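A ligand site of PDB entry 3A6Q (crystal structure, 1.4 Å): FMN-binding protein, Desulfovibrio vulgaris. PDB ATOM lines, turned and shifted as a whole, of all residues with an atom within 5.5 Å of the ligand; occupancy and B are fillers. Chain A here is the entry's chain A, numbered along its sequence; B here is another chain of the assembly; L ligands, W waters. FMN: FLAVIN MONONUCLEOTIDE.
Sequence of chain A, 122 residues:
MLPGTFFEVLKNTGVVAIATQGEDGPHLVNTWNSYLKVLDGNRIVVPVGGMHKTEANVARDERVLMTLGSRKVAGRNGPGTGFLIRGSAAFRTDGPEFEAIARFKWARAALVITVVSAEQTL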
ATOM      1  N   VAL A  15      20.132 -13.715   7.196  1.00  0.00           N
ATOM      2  CA  VAL A  15      19.869 -14.947   7.934  1.00  0.00           C
ATOM      3  C   VAL A  15      19.178 -14.632   9.260  1.00  0.00           C
ATOM      4  O   VAL A  15      19.700 -13.827  10.063  1.00  0.00           O
ATOM      5  CB  VAL A  15      21.183 -15.717   8.215  1.00  0.00           C
ATOM      6  CG1 VAL A  15      20.961 -16.912   9.128  1.00  0.00           C
ATOM      7  CG2 VAL A  15      21.889 -16.109   6.912  1.00  0.00           C
ATOM      8  N   HIS A  27      18.414 -24.521  21.680  1.00  0.00           N
ATOM      9  CA  HIS A  27      18.570 -24.937  20.301  1.00  0.00           C
ATOM     10  C   HIS A  27      18.488 -23.689  19.424  1.00  0.00           C
ATOM     11  O   HIS A  27      17.883 -22.677  19.819  1.00  0.00           O
ATOM     12  CB  HIS A  27      17.515 -25.984  19.892  1.00  0.00           C
ATOM     13  CG  HIS A  27      17.795 -26.633  18.576  1.00  0.00           C
ATOM     14  ND1 HIS A  27      19.057 -27.071  18.227  1.00  0.00           N
ATOM     15  CD2 HIS A  27      17.002 -26.872  17.504  1.00  0.00           C
ATOM     16  CE1 HIS A  27      19.018 -27.584  17.011  1.00  0.00           C
ATOM     17  NE2 HIS A  27      17.783 -27.482  16.543  1.00  0.00           N
ATOM     18  N   VAL A  29      18.033 -22.437  15.216  1.00  0.00           N
ATOM     19  CA  VAL A  29      17.714 -22.744  13.816  1.00  0.00           C
ATOM     20  C   VAL A  29      17.598 -21.438  13.030  1.00  0.00           C
ATOM     21  O   VAL A  29      17.643 -20.333  13.606  1.00  0.00           O
ATOM     22  CB  VAL A  29      16.478 -23.639  13.615  1.00  0.00           C
ATOM     23  CG1 VAL A  29      16.708 -25.015  14.292  1.00  0.00           C
ATOM     24  CG2 VAL A  29      15.195 -22.967  14.087  1.00  0.00           C
ATOM     25  N   ASN A  30      17.447 -21.560  11.723  1.00  0.00           N
ATOM     26  CA  ASN A  30      17.442 -20.395  10.838  1.00  0.00           C
ATOM     27  C   ASN A  30      16.296 -20.362   9.873  1.00  0.00           C
ATOM     28  O   ASN A  30      15.646 -21.376   9.555  1.00  0.00           O
ATOM     29  CB  ASN A  30      18.757 -20.335  10.048  1.00  0.00           C
ATOM     30  CG  ASN A  30      19.933 -20.231  10.939  1.00  0.00           C
ATOM     31  OD1 ASN A  30      20.738 -21.191  11.048  1.00  0.00           O
ATOM     32  ND2 ASN A  30      20.064 -19.097  11.635  1.00  0.00           N
ATOM     33  N   THR A  31      16.052 -19.149   9.397  1.00  0.00           N
ATOM     34  CA  THR A  31      15.330 -18.952   8.150  1.00  0.00           C
ATOM     35  C   THR A  31      15.978 -17.752   7.438  1.00  0.00           C
ATOM     36  O   THR A  31      17.045 -17.294   7.835  1.00  0.00           O
ATOM     37  CB  THR A  31      13.785 -18.833   8.343  1.00  0.00           C
ATOM     38  OG1 THR A  31      13.130 -18.858   7.062  1.00  0.00           O
ATOM     39  CG2 THR A  31      13.377 -17.577   9.136  1.00  0.00           C
ATOM     40  N   TRP A  32      15.335 -17.275   6.372  1.00  0.00           N
ATOM     41  CA  TRP A  32      15.826 -16.110   5.628  1.00  0.00           C
ATOM     42  C   TRP A  32      14.958 -14.899   5.890  1.00  0.00           C
ATOM     43  O   TRP A  32      13.733 -15.021   6.033  1.00  0.00           O
ATOM     44  CB  TRP A  32      15.809 -16.403   4.112  1.00  0.00           C
ATOM     45  CG  TRP A  32      16.677 -17.504   3.627  1.00  0.00           C
ATOM     46  CD1 TRP A  32      16.257 -18.723   3.195  1.00  0.00           C
ATOM     47  CD2 TRP A  32      18.100 -17.488   3.492  1.00  0.00           C
ATOM     48  NE1 TRP A  32      17.327 -19.488   2.811  1.00  0.00           N
ATOM     49  CE2 TRP A  32      18.482 -18.761   2.966  1.00  0.00           C
ATOM     50  CE3 TRP A  32      19.111 -16.546   3.760  1.00  0.00           C
ATOM     51  CZ2 TRP A  32      19.823 -19.084   2.694  1.00  0.00           C
ATOM     52  CZ3 TRP A  32      20.446 -16.884   3.482  1.00  0.00           C
ATOM     53  CH2 TRP A  32      20.789 -18.133   2.957  1.00  0.00           C
ATOM     54  N   TYR A  35      11.797 -14.743   3.839  1.00  0.00           N
ATOM     55  CA  TYR A  35      10.751 -15.738   4.082  1.00  0.00           C
ATOM     56  C   TYR A  35       9.760 -15.291   5.149  1.00  0.00           C
ATOM     57  O   TYR A  35       8.696 -15.885   5.246  1.00  0.00           O
ATOM     58  CB  TYR A  35      11.383 -17.050   4.528  1.00  0.00           C
ATOM     59  CG  TYR A  35      12.000 -17.893   3.440  1.00  0.00           C
ATOM     60  CD1 TYR A  35      12.248 -17.420   2.149  1.00  0.00           C
ATOM     61  CD2 TYR A  35      12.362 -19.214   3.746  1.00  0.00           C
ATOM     62  CE1 TYR A  35      12.847 -18.250   1.195  1.00  0.00           C
ATOM     63  CE2 TYR A  35      12.932 -20.028   2.798  1.00  0.00           C
ATOM     64  CZ  TYR A  35      13.169 -19.550   1.540  1.00  0.00           C
ATOM     65  OH  TYR A  35      13.740 -20.358   0.579  1.00  0.00           O
ATOM     66  N   VAL A  46       6.837 -18.008   9.854  1.00  0.00           N
ATOM     67  CA  VAL A  46       7.979 -18.630   9.193  1.00  0.00           C
ATOM     68  C   VAL A  46       7.529 -19.934   8.521  1.00  0.00           C
ATOM     69  O   VAL A  46       6.862 -20.755   9.177  1.00  0.00           O
ATOM     70  CB  VAL A  46       9.090 -18.978  10.245  1.00  0.00           C
ATOM     71  CG1 VAL A  46      10.287 -19.667   9.589  1.00  0.00           C
ATOM     72  CG2 VAL A  46       9.524 -17.758  11.073  1.00  0.00           C
ATOM     73  N   PRO A  47       7.888 -20.162   7.260  1.00  0.00           N
ATOM     74  CA  PRO A  47       7.604 -21.486   6.645  1.00  0.00           C
ATOM     75  C   PRO A  47       8.498 -22.576   7.261  1.00  0.00           C
ATOM     76  O   PRO A  47       9.718 -22.396   7.361  1.00  0.00           O
ATOM     77  CB  PRO A  47       7.913 -21.275   5.145  1.00  0.00           C
ATOM     78  CG  PRO A  47       8.984 -20.194   5.158  1.00  0.00           C
ATOM     79  CD  PRO A  47       8.612 -19.271   6.321  1.00  0.00           C
ATOM     80  N   VAL A  48       7.896 -23.696   7.647  1.00  0.00           N
ATOM     81  CA  VAL A  48       8.623 -24.780   8.307  1.00  0.00           C
ATOM     82  C   VAL A  48       8.739 -25.973   7.381  1.00  0.00           C
ATOM     83  O   VAL A  48       7.703 -26.553   6.990  1.00  0.00           O
ATOM     84  CB  VAL A  48       7.874 -25.209   9.565  1.00  0.00           C
ATOM     85  CG1 VAL A  48       8.542 -26.461  10.188  1.00  0.00           C
ATOM     86  CG2 VAL A  48       7.813 -24.058  10.568  1.00  0.00           C
ATOM     87  N   GLY A  49       9.971 -26.317   7.030  1.00  0.00           N
ATOM     88  CA  GLY A  49      10.243 -27.608   6.350  1.00  0.00           C
ATOM     89  C   GLY A  49      10.737 -28.657   7.330  1.00  0.00           C
ATOM     90  O   GLY A  49      10.180 -29.728   7.433  1.00  0.00           O
ATOM     91  N   GLY A  50      11.757 -28.299   8.105  1.00  0.00           N
ATOM     92  CA  GLY A  50      12.321 -29.169   9.150  1.00  0.00           C
ATOM     93  C   GLY A  50      11.772 -28.758  10.487  1.00  0.00           C
ATOM     94  O   GLY A  50      10.616 -29.000  10.805  1.00  0.00           O
ATOM     95  N   MET A  51      12.611 -28.115  11.294  1.00  0.00           N
ATOM     96  CA  MET A  51      12.251 -27.596  12.632  1.00  0.00           C
ATOM     97  C   MET A  51      11.556 -28.640  13.519  1.00  0.00           C
ATOM     98  O   MET A  51      10.610 -28.306  14.260  1.00  0.00           O
ATOM     99  CB  MET A  51      11.477 -26.276  12.544  1.00  0.00           C
ATOM    100  CG  MET A  51      12.299 -25.212  11.836  1.00  0.00           C
ATOM    101  SD  MET A  51      11.628 -23.568  12.130  1.00  0.00           S
ATOM    102  CE  MET A  51      12.680 -22.600  11.024  1.00  0.00           C
ATOM    103  N   HIS A  52      12.039 -29.877  13.458  1.00  0.00           N
ATOM    104  CA  HIS A  52      11.466 -30.932  14.297  1.00  0.00           C
ATOM    105  C   HIS A  52      11.909 -30.823  15.743  1.00  0.00           C
ATOM    106  O   HIS A  52      11.083 -30.929  16.648  1.00  0.00           O
ATOM    107  CB  HIS A  52      11.815 -32.311  13.721  1.00  0.00           C
ATOM    108  CG  HIS A  52      11.138 -32.575  12.421  1.00  0.00           C
ATOM    109  ND1 HIS A  52       9.790 -32.807  12.320  1.00  0.00           N
ATOM    110  CD2 HIS A  52      11.616 -32.588  11.149  1.00  0.00           C
ATOM    111  CE1 HIS A  52       9.469 -32.987  11.055  1.00  0.00           C
ATOM    112  NE2 HIS A  52      10.555 -32.853  10.319  1.00  0.00           N
ATOM    113  N   LYS A  53      13.194 -30.570  15.972  1.00  0.00           N
ATOM    114  CA  LYS A  53      13.660 -30.361  17.329  1.00  0.00           C
ATOM    115  C   LYS A  53      13.060 -29.047  17.881  1.00  0.00           C
ATOM    116  O   LYS A  53      12.562 -28.982  19.014  1.00  0.00           O
ATOM    117  CB  LYS A  53      15.181 -30.322  17.380  1.00  0.00           C
ATOM    118  CG  LYS A  53      15.727 -30.119  18.767  1.00  0.00           C
ATOM    119  CD  LYS A  53      17.230 -30.389  18.756  1.00  0.00           C
ATOM    120  CE  LYS A  53      17.866 -30.108  20.107  1.00  0.00           C
ATOM    121  NZ  LYS A  53      17.705 -31.230  21.043  1.00  0.00           N
ATOM    122  N   THR A  54      13.055 -28.012  17.036  1.00  0.00           N
ATOM    123  CA  THR A  54      12.456 -26.731  17.408  1.00  0.00           C
ATOM    124  C   THR A  54      10.972 -26.908  17.790  1.00  0.00           C
ATOM    125  O   THR A  54      10.542 -26.336  18.790  1.00  0.00           O
ATOM    126  CB  THR A  54      12.642 -25.745  16.236  1.00  0.00           C
ATOM    127  OG1 THR A  54      14.040 -25.499  16.054  1.00  0.00           O
ATOM    128  CG2 THR A  54      11.964 -24.433  16.512  1.00  0.00           C
ATOM    129  N   GLU A  55      10.232 -27.676  16.989  1.00  0.00           N
ATOM    130  CA  GLU A  55       8.812 -27.872  17.304  1.00  0.00           C
ATOM    131  C   GLU A  55       8.622 -28.605  18.645  1.00  0.00           C
ATOM    132  O   GLU A  55       7.735 -28.227  19.413  1.00  0.00           O
ATOM    133  CB  GLU A  55       8.136 -28.667  16.189  1.00  0.00           C
ATOM    134  CG  GLU A  55       6.627 -28.781  16.459  1.00  0.00           C
ATOM    135  CD  GLU A  55       5.859 -29.446  15.371  1.00  0.00           C
ATOM    136  OE1 GLU A  55       6.448 -29.951  14.386  1.00  0.00           O
ATOM    137  OE2 GLU A  55       4.614 -29.469  15.553  1.00  0.00           O
ATOM    138  N   TRP A 106       7.241 -26.739   0.051  1.00  0.00           N
ATOM    139  CA  TRP A 106       8.004 -27.578   0.976  1.00  0.00           C
ATOM    140  C   TRP A 106       7.589 -27.403   2.443  1.00  0.00           C
ATOM    141  O   TRP A 106       8.021 -28.158   3.310  1.00  0.00           O
ATOM    142  CB  TRP A 106       9.495 -27.338   0.779  1.00  0.00           C
ATOM    143  CG  TRP A 106       9.892 -25.891   0.806  1.00  0.00           C
ATOM    144  CD1 TRP A 106      10.105 -25.091  -0.264  1.00  0.00           C
ATOM    145  CD2 TRP A 106      10.151 -25.087   1.968  1.00  0.00           C
ATOM    146  NE1 TRP A 106      10.464 -23.829   0.146  1.00  0.00           N
ATOM    147  CE2 TRP A 106      10.518 -23.801   1.520  1.00  0.00           C
ATOM    148  CE3 TRP A 106      10.102 -25.340   3.350  1.00  0.00           C
ATOM    149  CZ2 TRP A 106      10.830 -22.740   2.404  1.00  0.00           C
ATOM    150  CZ3 TRP A 106      10.431 -24.293   4.237  1.00  0.00           C
ATOM    151  CH2 TRP A 106      10.797 -23.011   3.764  1.00  0.00           C
ATOM    152  N   LEU B  68      25.206 -18.915  11.173  1.00  0.00           N
ATOM    153  CA  LEU B  68      25.595 -17.878  10.208  1.00  0.00           C
ATOM    154  C   LEU B  68      25.352 -18.457   8.824  1.00  0.00           C
ATOM    155  O   LEU B  68      25.259 -19.682   8.641  1.00  0.00           O
ATOM    156  CB  LEU B  68      27.066 -17.460  10.385  1.00  0.00           C
ATOM    157  CG  LEU B  68      28.134 -18.464   9.982  1.00  0.00           C
ATOM    158  CD1 LEU B  68      29.469 -17.742   9.813  1.00  0.00           C
ATOM    159  CD2 LEU B  68      28.283 -19.619  10.974  1.00  0.00           C
ATOM    160  N   GLY B  69      25.296 -17.593   7.826  1.00  0.00           N
ATOM    161  CA  GLY B  69      24.999 -18.058   6.479  1.00  0.00           C
ATOM    162  C   GLY B  69      25.165 -16.977   5.458  1.00  0.00           C
ATOM    163  O   GLY B  69      25.589 -15.839   5.774  1.00  0.00           O
ATOM    164  N   THR B  81      23.252 -20.956   1.805  1.00  0.00           N
ATOM    165  CA  THR B  81      23.558 -21.948   2.826  1.00  0.00           C
ATOM    166  C   THR B  81      23.861 -21.321   4.162  1.00  0.00           C
ATOM    167  O   THR B  81      23.966 -20.099   4.276  1.00  0.00           O
ATOM    168  CB  THR B  81      24.734 -22.851   2.359  1.00  0.00           C
ATOM    169  OG1 THR B  81      24.773 -24.042   3.174  1.00  0.00           O
ATOM    170  CG2 THR B  81      26.079 -22.127   2.404  1.00  0.00           C
ATOM    171  N   GLY B  82      24.044 -22.184   5.156  1.00  0.00           N
ATOM    172  CA  GLY B  82      24.561 -21.722   6.447  1.00  0.00           C
ATOM    173  C   GLY B  82      24.878 -22.885   7.332  1.00  0.00           C
ATOM    174  O   GLY B  82      24.801 -24.040   6.896  1.00  0.00           O
ATOM    175  N   PHE B  83      25.315 -22.552   8.547  1.00  0.00           N
ATOM    176  CA  PHE B  83      25.906 -23.504   9.485  1.00  0.00           C
ATOM    177  C   PHE B  83      25.346 -23.349  10.872  1.00  0.00           C
ATOM    178  O   PHE B  83      25.063 -22.234  11.322  1.00  0.00           O
ATOM    179  CB  PHE B  83      27.438 -23.317   9.572  1.00  0.00           C
ATOM    180  CG  PHE B  83      28.126 -23.836   8.370  1.00  0.00           C
ATOM    181  CD1 PHE B  83      28.193 -23.085   7.224  1.00  0.00           C
ATOM    182  CD2 PHE B  83      28.671 -25.117   8.370  1.00  0.00           C
ATOM    183  CE1 PHE B  83      28.788 -23.617   6.054  1.00  0.00           C
ATOM    184  CE2 PHE B  83      29.265 -25.660   7.226  1.00  0.00           C
ATOM    185  CZ  PHE B  83      29.334 -24.880   6.075  1.00  0.00           C
ATOM    186  N   THR B 121      23.571 -26.724   7.370  1.00  0.00           N
ATOM    187  CA  THR B 121      22.162 -27.116   7.577  1.00  0.00           C
ATOM    188  C   THR B 121      21.264 -26.819   6.381  1.00  0.00           C
ATOM    189  O   THR B 121      20.037 -27.000   6.471  1.00  0.00           O
ATOM    190  CB  THR B 121      21.595 -26.424   8.820  1.00  0.00           C
ATOM    191  OG1 THR B 121      21.979 -25.053   8.718  1.00  0.00           O
ATOM    192  CG2 THR B 121      22.146 -27.006  10.124  1.00  0.00           C
ATOM    193  N   LEU B 122      21.849 -26.429   5.256  1.00  0.00           N
ATOM    194  CA  LEU B 122      21.107 -26.151   4.025  1.00  0.00           C
ATOM    195  C   LEU B 122      22.004 -26.493   2.814  1.00  0.00           C
ATOM    196  O   LEU B 122      23.204 -26.226   2.918  1.00  0.00           O
ATOM    197  CB  LEU B 122      20.615 -24.689   4.052  1.00  0.00           C
ATOM    198  CG  LEU B 122      19.859 -24.177   2.853  1.00  0.00           C
ATOM    199  CD1 LEU B 122      18.553 -24.944   2.625  1.00  0.00           C
ATOM    200  CD2 LEU B 122      19.562 -22.698   3.097  1.00  0.00           C
ATOM    201  OXT LEU B 122      21.541 -27.005   1.787  1.00  0.00           O
HETATM  202  N1  FMN L   1      14.395 -24.733   7.883  1.00  0.00           N
HETATM  203  C2  FMN L   1      13.033 -24.546   7.803  1.00  0.00           C
HETATM  204  O2  FMN L   1      12.252 -25.367   8.282  1.00  0.00           O
HETATM  205  N3  FMN L   1      12.552 -23.365   7.241  1.00  0.00           N
HETATM  206  C4  FMN L   1      13.403 -22.415   6.686  1.00  0.00           C
HETATM  207  O4  FMN L   1      12.869 -21.400   6.194  1.00  0.00           O
HETATM  208  C4A FMN L   1      14.762 -22.665   6.726  1.00  0.00           C
HETATM  209  N5  FMN L   1      15.619 -21.717   6.155  1.00  0.00           N
HETATM  210  C5A FMN L   1      16.976 -21.831   6.439  1.00  0.00           C
HETATM  211  C6  FMN L   1      17.812 -20.766   6.127  1.00  0.00           C
HETATM  212  C7  FMN L   1      19.153 -20.819   6.427  1.00  0.00           C
HETATM  213  C7M FMN L   1      20.069 -19.651   6.059  1.00  0.00           C
HETATM  214  C8  FMN L   1      19.681 -21.972   7.002  1.00  0.00           C
HETATM  215  C8M FMN L   1      21.164 -22.105   7.334  1.00  0.00           C
HETATM  216  C9  FMN L   1      18.834 -23.032   7.345  1.00  0.00           C
HETATM  217  C9A FMN L   1      17.480 -22.973   7.078  1.00  0.00           C
HETATM  218  N10 FMN L   1      16.610 -24.030   7.438  1.00  0.00           N
HETATM  219  C10 FMN L   1      15.250 -23.819   7.330  1.00  0.00           C
HETATM  220  C1' FMN L   1      17.083 -25.204   8.239  1.00  0.00           C
HETATM  221  C2' FMN L   1      16.856 -24.948   9.773  1.00  0.00           C
HETATM  222  O2' FMN L   1      17.768 -23.977  10.255  1.00  0.00           O
HETATM  223  C3' FMN L   1      17.071 -26.218  10.583  1.00  0.00           C
HETATM  224  O3' FMN L   1      18.400 -26.694  10.388  1.00  0.00           O
HETATM  225  C4' FMN L   1      16.117 -27.352  10.149  1.00  0.00           C
HETATM  226  O4' FMN L   1      14.775 -26.849   9.945  1.00  0.00           O
HETATM  227  C5' FMN L   1      16.083 -28.451  11.227  1.00  0.00           C
HETATM  228  O5' FMN L   1      15.453 -27.914  12.422  1.00  0.00           O
HETATM  229  P   FMN L   1      15.586 -28.660  13.856  1.00  0.00           P
HETATM  230  O1P FMN L   1      17.078 -28.708  14.184  1.00  0.00           O
HETATM  231  O2P FMN L   1      14.982 -30.087  13.665  1.00  0.00           O
HETATM  232  O3P FMN L   1      14.773 -27.832  14.789  1.00  0.00           O
HETATM  233  O   HOH W   1      18.654 -30.694  14.682  1.00  0.00           O
HETATM  234  O   HOH W   2      19.221 -27.676  12.840  1.00  0.00           O
HETATM  235  O   HOH W   3      20.479 -23.878  10.700  1.00  0.00           O
HETATM  236  O   HOH W   4      14.184 -31.402  11.603  1.00  0.00           O
HETATM  237  O   HOH W   5      18.958 -28.864   8.673  1.00  0.00           O
HETATM  238  O   HOH W   6      16.221 -32.354  14.545  1.00  0.00           O
HETATM  239  O   HOH W   7      15.101 -27.847   6.841  1.00  0.00           O
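Residues that only touch the ligand: Val 29 (3.5 Å), Trp 32 (3.4 Å), Tyr 35 (3.3 Å), Val 48 (3.7 Å), Trp 106 (3.6 Å), Gly 82 of chain B (3.5 Å), Thr 121 of chain B (3.4 Å) and Leu 122 of chain B (3.8 Å). Hydrophobic or aromatic side chains within 4 Å of the ligand: His 27, Val 29, Trp 32, Tyr 35, Met 51, His 52, Trp 106 and Leu 122 of chain B. 18 residues have an atom within 4 Å of the ligand: His 27, Val 29, Asn 30, Thr 31, Trp 32, Tyr 35, Pro 47, Val 48, Gly 49, Gly 50, Met 51, His 52, Lys 53, Thr 54, Trp 106, Gly 82 of chain B, Thr 121 of chain B and Leu 122 of chain B.
OG1 of Thr 81 of chain B sits at hydrogen-bond distance from O of Leu 122 of chain B (2.7 Å). N of Thr 121 of chain B lies within hydrogen-bond range of O of Gly 82 of chain B, at 3.0 Å.
Water W4 lies within hydrogen-bond range of O2P of the ligand (2.6 Å) and N of His 52 (3.2 Å). Water W3 lies within hydrogen-bond range of OD1 of Asn 30, O2' of the ligand and OG1 of Thr 121 of chain B. Water W5 bridges O3' of the ligand and O of Thr 121 of chain B.
N of Thr 54 lies within hydrogen-bond range of O3P of the ligand, 2.8 Å away. NE2 of His 27 sits at hydrogen-bond distance from O1P of the ligand (2.8 Å). An oxygen (O2P) of the ligand lies within hydrogen-bond range of the backbone NH (N) of Lys 53. N of Gly 49 sits at hydrogen-bond distance from O2 of the ligand (2.8 Å). An oxygen (O2P) of the ligand is in hydrogen-bond range of the backbone NH of His 52 (3.0 Å). An oxygen (O2') of the ligand lies close to the backbone carbonyl oxygen of Asn 30 (3.4 Å). The side-chain hydroxyl (OG1) of Thr 54 sits at hydrogen-bond distance from an oxygen (O3P) of the ligand, 2.8 Å away. N3 of the ligand sits at hydrogen-bond distance from O of Pro 47, 3.0 Å away. N of Met 51 lies within hydrogen-bond range of O4' of the ligand (2.8 Å). The backbone NH (N) of Asn 30 sits at hydrogen-bond distance from an oxygen (O2') of the ligand (2.8 Å). OG1 of Thr 31 sits at hydrogen-bond distance from O4 of the ligand. An oxygen (O2) of the ligand is in hydrogen-bond range of the backbone NH of Gly 50 (3.0 Å).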
